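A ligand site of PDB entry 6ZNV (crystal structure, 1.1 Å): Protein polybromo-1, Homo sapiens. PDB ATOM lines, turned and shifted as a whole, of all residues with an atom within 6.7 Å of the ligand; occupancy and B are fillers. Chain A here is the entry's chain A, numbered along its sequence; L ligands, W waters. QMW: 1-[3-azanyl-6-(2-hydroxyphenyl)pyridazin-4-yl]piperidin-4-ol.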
ATOM      1  N   LEU A  32     -18.577 -16.846   5.178  1.00  0.00           N
ATOM      2  CA  LEU A  32     -17.655 -17.188   4.101  1.00  0.00           C
ATOM      3  C   LEU A  32     -17.475 -16.047   3.108  1.00  0.00           C
ATOM      4  O   LEU A  32     -16.440 -15.960   2.440  1.00  0.00           O
ATOM      5  CB  LEU A  32     -18.129 -18.461   3.393  1.00  0.00           C
ATOM      6  CG  LEU A  32     -17.361 -18.981   2.174  1.00  0.00           C
ATOM      7  CD1 LEU A  32     -17.301 -20.496   2.202  1.00  0.00           C
ATOM      8  CD2 LEU A  32     -18.061 -18.520   0.901  1.00  0.00           C
ATOM      9  N   PHE A  33     -18.457 -15.169   2.986  1.00  0.00           N
ATOM     10  CA  PHE A  33     -18.468 -14.151   1.954  1.00  0.00           C
ATOM     11  C   PHE A  33     -17.857 -12.835   2.388  1.00  0.00           C
ATOM     12  O   PHE A  33     -17.809 -11.896   1.591  1.00  0.00           O
ATOM     13  CB  PHE A  33     -19.898 -13.930   1.451  1.00  0.00           C
ATOM     14  CG  PHE A  33     -20.544 -15.191   0.959  1.00  0.00           C
ATOM     15  CD1 PHE A  33     -20.099 -15.810  -0.191  1.00  0.00           C
ATOM     16  CD2 PHE A  33     -21.571 -15.782   1.673  1.00  0.00           C
ATOM     17  CE1 PHE A  33     -20.684 -16.985  -0.647  1.00  0.00           C
ATOM     18  CE2 PHE A  33     -22.167 -16.949   1.216  1.00  0.00           C
ATOM     19  CZ  PHE A  33     -21.722 -17.537   0.059  1.00  0.00           C
ATOM     20  N   GLN A  34     -17.357 -12.757   3.629  1.00  0.00           N
ATOM     21  CA  GLN A  34     -16.781 -11.503   4.102  1.00  0.00           C
ATOM     22  C   GLN A  34     -15.533 -11.132   3.305  1.00  0.00           C
ATOM     23  O   GLN A  34     -15.365  -9.973   2.894  1.00  0.00           O
ATOM     24  CB  GLN A  34     -16.428 -11.615   5.586  1.00  0.00           C
ATOM     25  CG  GLN A  34     -17.642 -11.482   6.493  1.00  0.00           C
ATOM     26  CD  GLN A  34     -18.089 -10.040   6.653  1.00  0.00           C
ATOM     27  OE1 GLN A  34     -17.541  -9.127   6.043  1.00  0.00           O
ATOM     28  NE2 GLN A  34     -19.112  -9.837   7.484  1.00  0.00           N
ATOM     29  N   LYS A  35     -14.657 -12.105   3.058  1.00  0.00           N
ATOM     30  CA  LYS A  35     -13.375 -11.844   2.426  1.00  0.00           C
ATOM     31  C   LYS A  35     -13.126 -12.862   1.321  1.00  0.00           C
ATOM     32  O   LYS A  35     -13.232 -14.074   1.545  1.00  0.00           O
ATOM     33  CB  LYS A  35     -12.234 -11.952   3.445  1.00  0.00           C
ATOM     34  CG  LYS A  35     -10.905 -11.480   2.912  1.00  0.00           C
ATOM     35  N   LEU A  36     -12.759 -12.360   0.144  1.00  0.00           N
ATOM     36  CA  LEU A  36     -12.403 -13.195  -1.002  1.00  0.00           C
ATOM     37  C   LEU A  36     -11.331 -14.211  -0.632  1.00  0.00           C
ATOM     38  O   LEU A  36     -10.493 -13.951   0.238  1.00  0.00           O
ATOM     39  CB  LEU A  36     -11.897 -12.330  -2.156  1.00  0.00           C
ATOM     40  CG  LEU A  36     -12.983 -11.644  -2.982  1.00  0.00           C
ATOM     41  CD1 LEU A  36     -12.360 -10.540  -3.797  1.00  0.00           C
ATOM     42  CD2 LEU A  36     -13.683 -12.658  -3.862  1.00  0.00           C
ATOM     43  N   PRO A  37     -11.332 -15.383  -1.269  1.00  0.00           N
ATOM     44  CA  PRO A  37     -10.302 -16.376  -0.972  1.00  0.00           C
ATOM     45  C   PRO A  37      -8.934 -15.923  -1.446  1.00  0.00           C
ATOM     46  O   PRO A  37      -8.796 -15.127  -2.386  1.00  0.00           O
ATOM     47  CB  PRO A  37     -10.772 -17.613  -1.740  1.00  0.00           C
ATOM     48  CG  PRO A  37     -11.583 -17.063  -2.855  1.00  0.00           C
ATOM     49  CD  PRO A  37     -12.261 -15.831  -2.311  1.00  0.00           C
ATOM     50  N   TYR A  42      -6.195 -20.241  -3.673  1.00  0.00           N
ATOM     51  CA  TYR A  42      -7.370 -20.508  -4.513  1.00  0.00           C
ATOM     52  C   TYR A  42      -7.251 -19.790  -5.852  1.00  0.00           C
ATOM     53  O   TYR A  42      -8.105 -18.977  -6.215  1.00  0.00           O
ATOM     54  CB  TYR A  42      -8.664 -20.184  -3.766  1.00  0.00           C
ATOM     55  CG  TYR A  42      -8.726 -21.068  -2.567  1.00  0.00           C
ATOM     56  CD1 TYR A  42      -9.132 -22.395  -2.691  1.00  0.00           C
ATOM     57  CD2 TYR A  42      -8.259 -20.643  -1.317  1.00  0.00           C
ATOM     58  CE1 TYR A  42      -9.101 -23.261  -1.599  1.00  0.00           C
ATOM     59  CE2 TYR A  42      -8.240 -21.482  -0.237  1.00  0.00           C
ATOM     60  CZ  TYR A  42      -8.650 -22.805  -0.374  1.00  0.00           C
ATOM     61  OH  TYR A  42      -8.617 -23.664   0.689  1.00  0.00           O
ATOM     62  N   TYR A  45     -10.167 -19.600  -8.511  1.00  0.00           N
ATOM     63  CA  TYR A  45     -11.254 -18.647  -8.321  1.00  0.00           C
ATOM     64  C   TYR A  45     -11.074 -17.446  -9.228  1.00  0.00           C
ATOM     65  O   TYR A  45     -12.035 -16.953  -9.848  1.00  0.00           O
ATOM     66  CB  TYR A  45     -11.338 -18.234  -6.848  1.00  0.00           C
ATOM     67  CG  TYR A  45     -12.589 -17.461  -6.537  1.00  0.00           C
ATOM     68  CD1 TYR A  45     -12.675 -16.091  -6.773  1.00  0.00           C
ATOM     69  CD2 TYR A  45     -13.718 -18.113  -6.092  1.00  0.00           C
ATOM     70  CE1 TYR A  45     -13.832 -15.394  -6.512  1.00  0.00           C
ATOM     71  CE2 TYR A  45     -14.893 -17.439  -5.847  1.00  0.00           C
ATOM     72  CZ  TYR A  45     -14.949 -16.073  -6.055  1.00  0.00           C
ATOM     73  OH  TYR A  45     -16.103 -15.356  -5.820  1.00  0.00           O
ATOM     74  N   ILE A  49     -13.611 -16.321 -12.080  1.00  0.00           N
ATOM     75  CA  ILE A  49     -14.449 -15.191 -11.685  1.00  0.00           C
ATOM     76  C   ILE A  49     -13.775 -13.919 -12.154  1.00  0.00           C
ATOM     77  O   ILE A  49     -12.737 -13.524 -11.612  1.00  0.00           O
ATOM     78  CB  ILE A  49     -14.674 -15.179 -10.161  1.00  0.00           C
ATOM     79  CG1 ILE A  49     -15.360 -16.470  -9.724  1.00  0.00           C
ATOM     80  CG2 ILE A  49     -15.439 -13.929  -9.730  1.00  0.00           C
ATOM     81  CD1 ILE A  49     -16.697 -16.734 -10.407  1.00  0.00           C
ATOM     82  N   ILE A  53     -15.707 -10.009  -5.817  1.00  0.00           N
ATOM     83  CA  ILE A  53     -16.244  -9.041  -4.870  1.00  0.00           C
ATOM     84  C   ILE A  53     -16.572  -9.788  -3.583  1.00  0.00           C
ATOM     85  O   ILE A  53     -16.915 -10.971  -3.608  1.00  0.00           O
ATOM     86  CB  ILE A  53     -17.488  -8.310  -5.444  1.00  0.00           C
ATOM     87  CG1 ILE A  53     -17.898  -7.137  -4.546  1.00  0.00           C
ATOM     88  CG2 ILE A  53     -18.632  -9.298  -5.649  1.00  0.00           C
ATOM     89  CD1 ILE A  53     -18.996  -6.280  -5.152  1.00  0.00           C
ATOM     90  N   ASP A  54     -16.478  -9.095  -2.443  1.00  0.00           N
ATOM     91  CA  ASP A  54     -16.825  -9.670  -1.156  1.00  0.00           C
ATOM     92  C   ASP A  54     -17.605  -8.645  -0.326  1.00  0.00           C
ATOM     93  O   ASP A  54     -17.791  -7.493  -0.724  1.00  0.00           O
ATOM     94  CB  ASP A  54     -15.594 -10.213  -0.409  1.00  0.00           C
ATOM     95  CG  ASP A  54     -14.475  -9.210  -0.316  1.00  0.00           C
ATOM     96  OD1 ASP A  54     -14.757  -7.984  -0.343  1.00  0.00           O
ATOM     97  OD2 ASP A  54     -13.307  -9.626  -0.187  1.00  0.00           O
ATOM     98  N   LEU A  55     -18.088  -9.087   0.833  1.00  0.00           N
ATOM     99  CA  LEU A  55     -18.847  -8.182   1.692  1.00  0.00           C
ATOM    100  C   LEU A  55     -17.975  -7.079   2.271  1.00  0.00           C
ATOM    101  O   LEU A  55     -18.458  -5.963   2.495  1.00  0.00           O
ATOM    102  CB  LEU A  55     -19.584  -8.939   2.793  1.00  0.00           C
ATOM    103  CG  LEU A  55     -20.683  -9.909   2.328  1.00  0.00           C
ATOM    104  CD1 LEU A  55     -21.168 -10.770   3.484  1.00  0.00           C
ATOM    105  CD2 LEU A  55     -21.846  -9.165   1.679  1.00  0.00           C
ATOM    106  N   LEU A  80     -21.915 -10.731  -6.240  1.00  0.00           N
ATOM    107  CA  LEU A  80     -21.325 -11.625  -5.240  1.00  0.00           C
ATOM    108  C   LEU A  80     -21.970 -13.002  -5.306  1.00  0.00           C
ATOM    109  O   LEU A  80     -21.290 -14.040  -5.368  1.00  0.00           O
ATOM    110  CB  LEU A  80     -21.506 -10.998  -3.860  1.00  0.00           C
ATOM    111  CG  LEU A  80     -20.655 -11.616  -2.768  1.00  0.00           C
ATOM    112  CD1 LEU A  80     -20.471 -10.615  -1.653  1.00  0.00           C
ATOM    113  CD2 LEU A  80     -21.256 -12.915  -2.260  1.00  0.00           C
ATOM    114  N   ALA A  81     -23.310 -13.038  -5.304  1.00  0.00           N
ATOM    115  CA  ALA A  81     -24.012 -14.309  -5.316  1.00  0.00           C
ATOM    116  C   ALA A  81     -23.783 -15.058  -6.614  1.00  0.00           C
ATOM    117  O   ALA A  81     -23.582 -16.272  -6.613  1.00  0.00           O
ATOM    118  CB  ALA A  81     -25.505 -14.071  -5.068  1.00  0.00           C
ATOM    119  N   ASN A  83     -21.199 -14.872  -8.614  1.00  0.00           N
ATOM    120  CA  ASN A  83     -19.836 -15.408  -8.570  1.00  0.00           C
ATOM    121  C   ASN A  83     -19.777 -16.691  -7.750  1.00  0.00           C
ATOM    122  O   ASN A  83     -19.189 -17.697  -8.166  1.00  0.00           O
ATOM    123  CB  ASN A  83     -18.895 -14.360  -7.959  1.00  0.00           C
ATOM    124  CG  ASN A  83     -18.610 -13.198  -8.893  1.00  0.00           C
ATOM    125  OD1 ASN A  83     -18.921 -13.236 -10.081  1.00  0.00           O
ATOM    126  ND2 ASN A  83     -17.984 -12.161  -8.344  1.00  0.00           N
ATOM    127  N   ALA A  84     -20.367 -16.658  -6.546  1.00  0.00           N
ATOM    128  CA  ALA A  84     -20.342 -17.834  -5.694  1.00  0.00           C
ATOM    129  C   ALA A  84     -21.074 -19.008  -6.342  1.00  0.00           C
ATOM    130  O   ALA A  84     -20.634 -20.150  -6.239  1.00  0.00           O
ATOM    131  CB  ALA A  84     -20.952 -17.504  -4.331  1.00  0.00           C
ATOM    132  N   LYS A  85     -22.194 -18.721  -7.011  1.00  0.00           N
ATOM    133  CA  LYS A  85     -22.953 -19.769  -7.676  1.00  0.00           C
ATOM    134  C   LYS A  85     -22.311 -20.252  -8.970  1.00  0.00           C
ATOM    135  O   LYS A  85     -22.741 -21.280  -9.499  1.00  0.00           O
ATOM    136  CB  LYS A  85     -24.385 -19.276  -7.926  1.00  0.00           C
ATOM    137  CG  LYS A  85     -25.195 -19.162  -6.641  1.00  0.00           C
ATOM    138  CD  LYS A  85     -26.372 -18.202  -6.766  1.00  0.00           C
ATOM    139  CE  LYS A  85     -27.373 -18.694  -7.790  1.00  0.00           C
ATOM    140  NZ  LYS A  85     -28.550 -17.773  -7.842  1.00  0.00           N
ATOM    141  N   TYR A  87     -18.734 -20.527  -9.080  1.00  0.00           N
ATOM    142  CA  TYR A  87     -17.567 -21.281  -8.611  1.00  0.00           C
ATOM    143  C   TYR A  87     -17.973 -22.556  -7.894  1.00  0.00           C
ATOM    144  O   TYR A  87     -17.211 -23.537  -7.911  1.00  0.00           O
ATOM    145  CB  TYR A  87     -16.762 -20.393  -7.668  1.00  0.00           C
ATOM    146  CG  TYR A  87     -15.440 -20.984  -7.245  1.00  0.00           C
ATOM    147  CD1 TYR A  87     -14.359 -21.028  -8.132  1.00  0.00           C
ATOM    148  CD2 TYR A  87     -15.246 -21.494  -5.964  1.00  0.00           C
ATOM    149  CE1 TYR A  87     -13.144 -21.567  -7.762  1.00  0.00           C
ATOM    150  CE2 TYR A  87     -14.030 -22.042  -5.589  1.00  0.00           C
ATOM    151  CZ  TYR A  87     -12.993 -22.062  -6.487  1.00  0.00           C
ATOM    152  OH  TYR A  87     -11.785 -22.595  -6.105  1.00  0.00           O
ATOM    153  N   ASN A  88     -19.138 -22.571  -7.258  1.00  0.00           N
ATOM    154  CA  ASN A  88     -19.552 -23.671  -6.413  1.00  0.00           C
ATOM    155  C   ASN A  88     -20.692 -24.454  -7.050  1.00  0.00           C
ATOM    156  O   ASN A  88     -21.530 -23.884  -7.761  1.00  0.00           O
ATOM    157  CB  ASN A  88     -19.997 -23.156  -5.040  1.00  0.00           C
ATOM    158  CG  ASN A  88     -18.861 -22.503  -4.285  1.00  0.00           C
ATOM    159  OD1 ASN A  88     -18.078 -23.185  -3.620  1.00  0.00           O
ATOM    160  ND2 ASN A  88     -18.750 -21.187  -4.390  1.00  0.00           N
ATOM    161  N   VAL A  94     -22.178 -23.457  -0.027  1.00  0.00           N
ATOM    162  CA  VAL A  94     -21.865 -22.094  -0.431  1.00  0.00           C
ATOM    163  C   VAL A  94     -22.879 -21.587  -1.444  1.00  0.00           C
ATOM    164  O   VAL A  94     -23.327 -20.431  -1.380  1.00  0.00           O
ATOM    165  CB  VAL A  94     -20.421 -21.997  -0.974  1.00  0.00           C
ATOM    166  CG1 VAL A  94     -20.150 -20.602  -1.517  1.00  0.00           C
ATOM    167  CG2 VAL A  94     -19.422 -22.366   0.121  1.00  0.00           C
HETATM  168  C1  QMW L   1     -16.066 -17.901  -2.016  1.00  0.00           C
HETATM  169  C2  QMW L   1     -16.350 -16.450  -1.971  1.00  0.00           C
HETATM  170  N3  QMW L   1     -14.073 -20.640  -0.498  1.00  0.00           N
HETATM  171  C4  QMW L   1     -16.156 -14.317  -0.836  1.00  0.00           C
HETATM  172  C5  QMW L   1     -16.962 -13.726  -1.781  1.00  0.00           C
HETATM  173  C6  QMW L   1     -17.470 -14.475  -2.820  1.00  0.00           C
HETATM  174  C7  QMW L   1     -17.166 -15.819  -2.925  1.00  0.00           C
HETATM  175  C9  QMW L   1     -15.001 -19.895  -1.270  1.00  0.00           C
HETATM  176  C10 QMW L   1     -13.530 -20.011   0.711  1.00  0.00           C
HETATM  177  C12 QMW L   1     -11.890 -21.878   0.922  1.00  0.00           C
HETATM  178  C13 QMW L   1     -12.433 -22.460  -0.365  1.00  0.00           C
HETATM  179  C14 QMW L   1     -13.028 -21.354  -1.235  1.00  0.00           C
HETATM  180  N   QMW L   1     -15.802 -21.927  -2.317  1.00  0.00           N
HETATM  181  C   QMW L   1     -15.815 -20.596  -2.189  1.00  0.00           C
HETATM  182  O   QMW L   1     -17.646 -16.539  -3.979  1.00  0.00           O
HETATM  183  C11 QMW L   1     -12.944 -21.062   1.637  1.00  0.00           C
HETATM  184  C3  QMW L   1     -15.848 -15.665  -0.928  1.00  0.00           C
HETATM  185  C8  QMW L   1     -15.137 -18.515  -1.176  1.00  0.00           C
HETATM  186  N1  QMW L   1     -16.662 -19.947  -2.982  1.00  0.00           N
HETATM  187  N2  QMW L   1     -16.795 -18.608  -2.900  1.00  0.00           N
HETATM  188  O1  QMW L   1     -11.418 -22.935   1.758  1.00  0.00           O
HETATM  189  O   HOH W   1     -15.797 -24.450  -0.417  1.00  0.00           O
HETATM  190  O   HOH W   2      -9.778 -21.634   3.233  1.00  0.00           O
HETATM  191  O   HOH W   3     -16.833 -12.702  -5.752  1.00  0.00           O
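Merely in contact with the ligand: Ile 53 (3.3 Å), Leu 32 (3.4 Å), Ala 84 (3.4 Å), Phe 33 (3.6 Å), Tyr 87 (3.6 Å), Lys 35 (3.8 Å), Val 94 (3.8 Å), Pro 37 (3.8 Å) and Leu 36 (3.9 Å). Of the 20 residues printed, 12 come within 4 Å of the ligand.
O of the ligand sits at hydrogen-bond distance from OH of Tyr 45 (2.7 Å). ND2 of Asn 88 lies within hydrogen-bond range of N1 of the ligand, 2.8 Å away. The side-chain hydroxyl (OH) of Tyr 42 is in hydrogen-bond range of an oxygen (O1) of the ligand.
Water W2 bridges an oxygen (O1) of the ligand and the side-chain hydroxyl of Tyr 42. Water W3 lies within hydrogen-bond range of the side-chain hydroxyl (OH) of Tyr 45 (2.8 Å), the backbone carbonyl oxygen (O) of Ile 53 (2.8 Å) and the side-chain amide nitrogen (ND2) of Asn 83 (2.9 Å).
ND2 of Asn 88 sits at hydrogen-bond distance from O of Ala 84, at 2.8 Å. The backbone carbonyl oxygen (O) of Phe 33 is in hydrogen-bond range of the backbone NH (N) of Leu 55. The backbone NH (N) of Leu 36 lies within hydrogen-bond range of the side-chain carboxylate (OD2) of Asp 54, at 2.8 Å.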
